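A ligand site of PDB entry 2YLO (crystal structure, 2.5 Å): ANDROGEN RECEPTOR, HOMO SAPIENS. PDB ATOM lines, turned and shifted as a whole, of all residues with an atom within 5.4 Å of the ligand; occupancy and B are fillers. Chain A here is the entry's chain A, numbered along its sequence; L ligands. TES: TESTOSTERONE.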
ATOM      1  N   LEU A  38     -20.071  17.564  12.862  1.00  0.00           N
ATOM      2  CA  LEU A  38     -20.432  16.176  13.174  1.00  0.00           C
ATOM      3  C   LEU A  38     -21.796  15.743  12.610  1.00  0.00           C
ATOM      4  O   LEU A  38     -21.887  14.647  12.057  1.00  0.00           O
ATOM      5  CB  LEU A  38     -20.224  15.836  14.661  1.00  0.00           C
ATOM      6  CG  LEU A  38     -18.849  15.202  15.002  1.00  0.00           C
ATOM      7  CD1 LEU A  38     -18.769  13.817  14.396  1.00  0.00           C
ATOM      8  CD2 LEU A  38     -17.626  16.067  14.584  1.00  0.00           C
ATOM      9  N   LEU A  41     -21.085  15.018   8.938  1.00  0.00           N
ATOM     10  CA  LEU A  41     -20.403  13.706   8.828  1.00  0.00           C
ATOM     11  C   LEU A  41     -21.370  12.541   9.003  1.00  0.00           C
ATOM     12  O   LEU A  41     -21.333  11.558   8.252  1.00  0.00           O
ATOM     13  CB  LEU A  41     -19.252  13.565   9.838  1.00  0.00           C
ATOM     14  CG  LEU A  41     -17.953  14.268   9.496  1.00  0.00           C
ATOM     15  CD1 LEU A  41     -16.947  14.123  10.625  1.00  0.00           C
ATOM     16  CD2 LEU A  41     -17.384  13.706   8.177  1.00  0.00           C
ATOM     17  N   ASN A  42     -22.241  12.646   9.998  1.00  0.00           N
ATOM     18  CA  ASN A  42     -23.341  11.694  10.132  1.00  0.00           C
ATOM     19  C   ASN A  42     -24.192  11.546   8.882  1.00  0.00           C
ATOM     20  O   ASN A  42     -24.452  10.419   8.450  1.00  0.00           O
ATOM     21  CB  ASN A  42     -24.198  12.024  11.335  1.00  0.00           C
ATOM     22  CG  ASN A  42     -23.469  11.766  12.639  1.00  0.00           C
ATOM     23  OD1 ASN A  42     -22.393  11.133  12.679  1.00  0.00           O
ATOM     24  ND2 ASN A  42     -24.035  12.275  13.719  1.00  0.00           N
ATOM     25  N   LEU A  44     -23.405  12.451   5.774  1.00  0.00           N
ATOM     26  CA  LEU A  44     -22.502  11.786   4.824  1.00  0.00           C
ATOM     27  C   LEU A  44     -22.508  10.269   5.010  1.00  0.00           C
ATOM     28  O   LEU A  44     -22.695   9.524   4.042  1.00  0.00           O
ATOM     29  CB  LEU A  44     -21.071  12.313   4.955  1.00  0.00           C
ATOM     30  CG  LEU A  44     -20.080  11.849   3.881  1.00  0.00           C
ATOM     31  CD1 LEU A  44     -20.583  12.115   2.444  1.00  0.00           C
ATOM     32  CD2 LEU A  44     -18.697  12.454   4.108  1.00  0.00           C
ATOM     33  N   GLY A  45     -22.347   9.824   6.263  1.00  0.00           N
ATOM     34  CA  GLY A  45     -22.447   8.413   6.607  1.00  0.00           C
ATOM     35  C   GLY A  45     -23.711   7.784   6.061  1.00  0.00           C
ATOM     36  O   GLY A  45     -23.620   6.874   5.243  1.00  0.00           O
ATOM     37  N   GLN A  48     -23.757   7.738   2.079  1.00  0.00           N
ATOM     38  CA  GLN A  48     -22.766   6.772   1.611  1.00  0.00           C
ATOM     39  C   GLN A  48     -23.200   5.320   1.881  1.00  0.00           C
ATOM     40  O   GLN A  48     -22.739   4.410   1.199  1.00  0.00           O
ATOM     41  CB  GLN A  48     -21.401   7.029   2.254  1.00  0.00           C
ATOM     42  CG  GLN A  48     -20.742   8.346   1.892  1.00  0.00           C
ATOM     43  CD  GLN A  48     -19.624   8.222   0.850  1.00  0.00           C
ATOM     44  OE1 GLN A  48     -18.676   9.027   0.835  1.00  0.00           O
ATOM     45  NE2 GLN A  48     -19.743   7.215  -0.038  1.00  0.00           N
ATOM     46  N   TRP A  78     -18.822  -1.303   7.285  1.00  0.00           N
ATOM     47  CA  TRP A  78     -18.922   0.026   6.697  1.00  0.00           C
ATOM     48  C   TRP A  78     -17.817   1.063   7.027  1.00  0.00           C
ATOM     49  O   TRP A  78     -17.145   1.537   6.121  1.00  0.00           O
ATOM     50  CB  TRP A  78     -20.296   0.600   6.891  1.00  0.00           C
ATOM     51  CG  TRP A  78     -20.670   0.700   8.303  1.00  0.00           C
ATOM     52  CD1 TRP A  78     -21.183  -0.293   9.070  1.00  0.00           C
ATOM     53  CD2 TRP A  78     -20.594   1.861   9.129  1.00  0.00           C
ATOM     54  NE1 TRP A  78     -21.428   0.173  10.343  1.00  0.00           N
ATOM     55  CE2 TRP A  78     -21.079   1.488  10.405  1.00  0.00           C
ATOM     56  CE3 TRP A  78     -20.172   3.180   8.933  1.00  0.00           C
ATOM     57  CZ2 TRP A  78     -21.131   2.381  11.489  1.00  0.00           C
ATOM     58  CZ3 TRP A  78     -20.239   4.067   9.999  1.00  0.00           C
ATOM     59  CH2 TRP A  78     -20.724   3.664  11.253  1.00  0.00           C
ATOM     60  N   MET A  79     -17.627   1.418   8.302  1.00  0.00           N
ATOM     61  CA  MET A  79     -16.475   2.257   8.752  1.00  0.00           C
ATOM     62  C   MET A  79     -15.192   1.957   7.983  1.00  0.00           C
ATOM     63  O   MET A  79     -14.635   2.835   7.342  1.00  0.00           O
ATOM     64  CB  MET A  79     -16.196   2.096  10.259  1.00  0.00           C
ATOM     65  CG  MET A  79     -15.416   3.252  10.872  1.00  0.00           C
ATOM     66  SD  MET A  79     -16.389   4.778  10.970  1.00  0.00           S
ATOM     67  CE  MET A  79     -17.418   4.462  12.381  1.00  0.00           C
ATOM     68  N   MET A  82     -15.581   2.968   4.142  1.00  0.00           N
ATOM     69  CA  MET A  82     -15.654   4.400   3.954  1.00  0.00           C
ATOM     70  C   MET A  82     -14.359   5.142   4.279  1.00  0.00           C
ATOM     71  O   MET A  82     -13.921   6.007   3.527  1.00  0.00           O
ATOM     72  CB  MET A  82     -16.855   4.929   4.695  1.00  0.00           C
ATOM     73  CG  MET A  82     -18.131   4.270   4.220  1.00  0.00           C
ATOM     74  SD  MET A  82     -19.497   4.877   5.200  1.00  0.00           S
ATOM     75  CE  MET A  82     -20.916   4.093   4.447  1.00  0.00           C
ATOM     76  N   VAL A  83     -13.701   4.753   5.362  1.00  0.00           N
ATOM     77  CA  VAL A  83     -12.368   5.314   5.697  1.00  0.00           C
ATOM     78  C   VAL A  83     -11.320   5.064   4.587  1.00  0.00           C
ATOM     79  O   VAL A  83     -10.594   5.969   4.193  1.00  0.00           O
ATOM     80  CB  VAL A  83     -11.863   4.744   7.030  1.00  0.00           C
ATOM     81  CG1 VAL A  83     -10.452   5.169   7.268  1.00  0.00           C
ATOM     82  CG2 VAL A  83     -12.720   5.250   8.163  1.00  0.00           C
ATOM     83  N   MET A  86     -12.152   7.032   1.418  1.00  0.00           N
ATOM     84  CA  MET A  86     -11.928   8.467   1.726  1.00  0.00           C
ATOM     85  C   MET A  86     -10.414   8.775   1.764  1.00  0.00           C
ATOM     86  O   MET A  86      -9.989   9.799   1.251  1.00  0.00           O
ATOM     87  CB  MET A  86     -12.681   8.896   2.988  1.00  0.00           C
ATOM     88  CG  MET A  86     -12.532  10.375   3.344  1.00  0.00           C
ATOM     89  SD  MET A  86     -10.942  10.753   4.158  1.00  0.00           S
ATOM     90  CE  MET A  86     -11.328  10.488   5.872  1.00  0.00           C
ATOM     91  N   ARG A  89      -9.756   9.027  -2.061  1.00  0.00           N
ATOM     92  CA  ARG A  89     -10.249  10.341  -2.516  1.00  0.00           C
ATOM     93  C   ARG A  89      -9.308  11.449  -2.089  1.00  0.00           C
ATOM     94  O   ARG A  89      -9.113  12.415  -2.809  1.00  0.00           O
ATOM     95  CB  ARG A  89     -11.619  10.696  -1.930  1.00  0.00           C
ATOM     96  CG  ARG A  89     -12.767   9.847  -2.402  1.00  0.00           C
ATOM     97  CD  ARG A  89     -14.105  10.545  -2.154  1.00  0.00           C
ATOM     98  NE  ARG A  89     -14.453  10.711  -0.731  1.00  0.00           N
ATOM     99  CZ  ARG A  89     -15.083   9.794   0.001  1.00  0.00           C
ATOM    100  NH1 ARG A  89     -15.403   8.632  -0.544  1.00  0.00           N
ATOM    101  NH2 ARG A  89     -15.375  10.014   1.285  1.00  0.00           N
ATOM    102  N   PHE A 101     -13.510  14.330   2.703  1.00  0.00           N
ATOM    103  CA  PHE A 101     -14.732  13.611   3.030  1.00  0.00           C
ATOM    104  C   PHE A 101     -15.746  13.626   1.893  1.00  0.00           C
ATOM    105  O   PHE A 101     -16.356  12.617   1.616  1.00  0.00           O
ATOM    106  CB  PHE A 101     -15.339  14.079   4.359  1.00  0.00           C
ATOM    107  CG  PHE A 101     -14.532  13.656   5.545  1.00  0.00           C
ATOM    108  CD1 PHE A 101     -13.487  14.455   6.022  1.00  0.00           C
ATOM    109  CD2 PHE A 101     -14.777  12.438   6.164  1.00  0.00           C
ATOM    110  CE1 PHE A 101     -12.733  14.045   7.137  1.00  0.00           C
ATOM    111  CE2 PHE A 101     -14.042  12.033   7.283  1.00  0.00           C
ATOM    112  CZ  PHE A 101     -13.020  12.816   7.763  1.00  0.00           C
ATOM    113  N   MET A 117     -12.091  15.332  16.860  1.00  0.00           N
ATOM    114  CA  MET A 117     -11.432  14.047  16.664  1.00  0.00           C
ATOM    115  C   MET A 117     -10.140  14.214  15.938  1.00  0.00           C
ATOM    116  O   MET A 117      -9.917  13.611  14.904  1.00  0.00           O
ATOM    117  CB  MET A 117     -12.335  13.001  16.000  1.00  0.00           C
ATOM    118  CG  MET A 117     -13.429  13.533  15.141  1.00  0.00           C
ATOM    119  SD  MET A 117     -13.778  12.289  13.911  1.00  0.00           S
ATOM    120  CE  MET A 117     -13.395  13.191  12.428  1.00  0.00           C
ATOM    121  N   MET A 124      -6.240   8.812   9.926  1.00  0.00           N
ATOM    122  CA  MET A 124      -6.849   8.749   8.607  1.00  0.00           C
ATOM    123  C   MET A 124      -5.932   9.403   7.547  1.00  0.00           C
ATOM    124  O   MET A 124      -5.704   8.811   6.472  1.00  0.00           O
ATOM    125  CB  MET A 124      -8.222   9.360   8.610  1.00  0.00           C
ATOM    126  CG  MET A 124      -9.161   8.566   9.439  1.00  0.00           C
ATOM    127  SD  MET A 124     -10.880   9.101   9.297  1.00  0.00           S
ATOM    128  CE  MET A 124     -11.010  10.393  10.527  1.00  0.00           C
ATOM    129  N   LEU A 210     -12.725   4.940  15.626  1.00  0.00           N
ATOM    130  CA  LEU A 210     -13.867   5.684  15.147  1.00  0.00           C
ATOM    131  C   LEU A 210     -15.190   5.075  15.582  1.00  0.00           C
ATOM    132  O   LEU A 210     -16.202   5.772  15.647  1.00  0.00           O
ATOM    133  CB  LEU A 210     -13.872   5.717  13.631  1.00  0.00           C
ATOM    134  CG  LEU A 210     -12.797   6.481  12.887  1.00  0.00           C
ATOM    135  CD1 LEU A 210     -12.947   6.216  11.416  1.00  0.00           C
ATOM    136  CD2 LEU A 210     -12.939   7.950  13.204  1.00  0.00           C
ATOM    137  N   PHE A 213     -15.407   6.386  19.114  1.00  0.00           N
ATOM    138  CA  PHE A 213     -15.806   7.771  19.003  1.00  0.00           C
ATOM    139  C   PHE A 213     -17.312   7.960  18.715  1.00  0.00           C
ATOM    140  O   PHE A 213     -18.011   8.536  19.529  1.00  0.00           O
ATOM    141  CB  PHE A 213     -14.993   8.507  17.968  1.00  0.00           C
ATOM    142  CG  PHE A 213     -15.156  10.010  18.037  1.00  0.00           C
ATOM    143  CD1 PHE A 213     -14.560  10.730  19.050  1.00  0.00           C
ATOM    144  CD2 PHE A 213     -15.892  10.674  17.121  1.00  0.00           C
ATOM    145  CE1 PHE A 213     -14.693  12.103  19.144  1.00  0.00           C
ATOM    146  CE2 PHE A 213     -16.040  12.041  17.197  1.00  0.00           C
ATOM    147  CZ  PHE A 213     -15.419  12.765  18.226  1.00  0.00           C
ATOM    148  N   THR A 214     -17.783   7.463  17.583  1.00  0.00           N
ATOM    149  CA  THR A 214     -19.141   7.707  17.200  1.00  0.00           C
ATOM    150  C   THR A 214     -20.140   7.132  18.240  1.00  0.00           C
ATOM    151  O   THR A 214     -21.148   7.770  18.534  1.00  0.00           O
ATOM    152  CB  THR A 214     -19.417   7.295  15.712  1.00  0.00           C
ATOM    153  OG1 THR A 214     -20.765   7.638  15.334  1.00  0.00           O
ATOM    154  CG2 THR A 214     -19.152   5.808  15.462  1.00  0.00           C
ATOM    155  N   LEU A 217     -20.316   9.533  21.038  1.00  0.00           N
ATOM    156  CA  LEU A 217     -21.078  10.649  20.526  1.00  0.00           C
ATOM    157  C   LEU A 217     -22.583  10.397  20.583  1.00  0.00           C
ATOM    158  O   LEU A 217     -23.350  11.224  21.061  1.00  0.00           O
ATOM    159  CB  LEU A 217     -20.679  10.953  19.098  1.00  0.00           C
ATOM    160  CG  LEU A 217     -21.189  12.321  18.661  1.00  0.00           C
ATOM    161  CD1 LEU A 217     -20.717  13.436  19.644  1.00  0.00           C
ATOM    162  CD2 LEU A 217     -20.788  12.635  17.233  1.00  0.00           C
ATOM    163  N   PHE A 228     -28.095  12.320  14.576  1.00  0.00           N
ATOM    164  CA  PHE A 228     -27.821  11.061  13.883  1.00  0.00           C
ATOM    165  C   PHE A 228     -29.064  10.661  13.105  1.00  0.00           C
ATOM    166  O   PHE A 228     -30.155  10.561  13.677  1.00  0.00           O
ATOM    167  CB  PHE A 228     -27.433   9.956  14.852  1.00  0.00           C
ATOM    168  CG  PHE A 228     -26.012  10.014  15.296  1.00  0.00           C
ATOM    169  CD1 PHE A 228     -25.625  10.879  16.318  1.00  0.00           C
ATOM    170  CD2 PHE A 228     -25.053   9.212  14.713  1.00  0.00           C
ATOM    171  CE1 PHE A 228     -24.310  10.939  16.752  1.00  0.00           C
ATOM    172  CE2 PHE A 228     -23.703   9.255  15.129  1.00  0.00           C
ATOM    173  CZ  PHE A 228     -23.327  10.113  16.152  1.00  0.00           C
ATOM    174  N   MET A 232     -28.111   5.477  10.744  1.00  0.00           N
ATOM    175  CA  MET A 232     -26.821   5.645  11.466  1.00  0.00           C
ATOM    176  C   MET A 232     -27.020   5.440  12.966  1.00  0.00           C
ATOM    177  O   MET A 232     -26.219   4.781  13.626  1.00  0.00           O
ATOM    178  CB  MET A 232     -26.193   6.997  11.173  1.00  0.00           C
ATOM    179  CG  MET A 232     -25.584   7.051   9.800  1.00  0.00           C
ATOM    180  SD  MET A 232     -23.896   6.368   9.672  1.00  0.00           S
ATOM    181  CE  MET A 232     -23.039   7.672  10.577  1.00  0.00           C
ATOM    182  N   ILE A 236     -25.400   2.247  14.911  1.00  0.00           N
ATOM    183  CA  ILE A 236     -24.429   2.552  15.926  1.00  0.00           C
ATOM    184  C   ILE A 236     -24.803   2.020  17.292  1.00  0.00           C
ATOM    185  O   ILE A 236     -23.924   1.678  18.083  1.00  0.00           O
ATOM    186  CB  ILE A 236     -23.978   4.024  15.878  1.00  0.00           C
ATOM    187  CG1 ILE A 236     -23.040   4.168  14.655  1.00  0.00           C
ATOM    188  CG2 ILE A 236     -23.309   4.442  17.192  1.00  0.00           C
ATOM    189  CD1 ILE A 236     -23.095   5.503  13.927  1.00  0.00           C
HETATM  190  C1  TES L   1     -18.460   9.181   6.598  1.00  0.00           C
HETATM  191  C2  TES L   1     -17.906   9.024   5.158  1.00  0.00           C
HETATM  192  C3  TES L   1     -16.384   8.956   5.096  1.00  0.00           C
HETATM  193  O3  TES L   1     -15.772   9.213   4.053  1.00  0.00           O
HETATM  194  C4  TES L   1     -15.601   8.569   6.278  1.00  0.00           C
HETATM  195  C5  TES L   1     -16.142   8.485   7.504  1.00  0.00           C
HETATM  196  C6  TES L   1     -15.142   8.300   8.641  1.00  0.00           C
HETATM  197  C7  TES L   1     -15.588   9.180   9.787  1.00  0.00           C
HETATM  198  C8  TES L   1     -17.035   8.935  10.180  1.00  0.00           C
HETATM  199  C9  TES L   1     -18.001   9.246   9.036  1.00  0.00           C
HETATM  200  C10 TES L   1     -17.659   8.505   7.746  1.00  0.00           C
HETATM  201  C11 TES L   1     -19.499   9.063   9.422  1.00  0.00           C
HETATM  202  C12 TES L   1     -19.893   9.805  10.712  1.00  0.00           C
HETATM  203  C13 TES L   1     -18.907   9.470  11.820  1.00  0.00           C
HETATM  204  C14 TES L   1     -17.456   9.766  11.400  1.00  0.00           C
HETATM  205  C15 TES L   1     -16.648   9.697  12.703  1.00  0.00           C
HETATM  206  C16 TES L   1     -17.641  10.223  13.762  1.00  0.00           C
HETATM  207  C17 TES L   1     -19.026  10.330  13.067  1.00  0.00           C
HETATM  208  O17 TES L   1     -20.111   9.893  13.899  1.00  0.00           O
HETATM  209  C18 TES L   1     -19.063   7.969  12.127  1.00  0.00           C
HETATM  210  C19 TES L   1     -18.165   7.074   7.847  1.00  0.00           C
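The side-chain hydroxyl (OG1) of Thr 214 sits at hydrogen-bond distance from an oxygen (O17) of the ligand (2.8 Å).
OD1 of Asn 42 lies within hydrogen-bond range of O17 of the ligand.
NH2 of Arg 89 is in hydrogen-bond range of O3 of the ligand.
The backbone carbonyl oxygen (O) of Phe 101 sits at hydrogen-bond distance from the guanidinium group (NH2) of Arg 89.
NH2 of Arg 89 is in hydrogen-bond range of OE1 of Gln 48 (3.5 Å).
Leu 38 touches the ligand.
Leu 41 touches the ligand (O to C11, 3.3 Å).
Leu 44 touches the ligand.
Gly 45 touches the ligand (N to C1, 3.95 Å).
Met 79 touches the ligand (CE to C18, 3.9 Å).
Met 82 touches the ligand (SD to C19, 3.7 Å).
Val 83 touches the ligand.
Met 86 touches the ligand.
CE2 of Phe 101 touches C4 of the ligand, 3.9 Å away.
Phe 213 touches the ligand.
Phe 228 touches the ligand (CE2 to O17, 3.8 Å).
Met 232 touches the ligand.
15 residues have an atom within 4 Å of the ligand: Leu 38, Leu 41, Asn 42, Leu 44, Gly 45, Met 79, Met 82, Val 83, Met 86, Arg 89, Phe 101, Phe 213, Thr 214, Phe 228 and Met 232.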
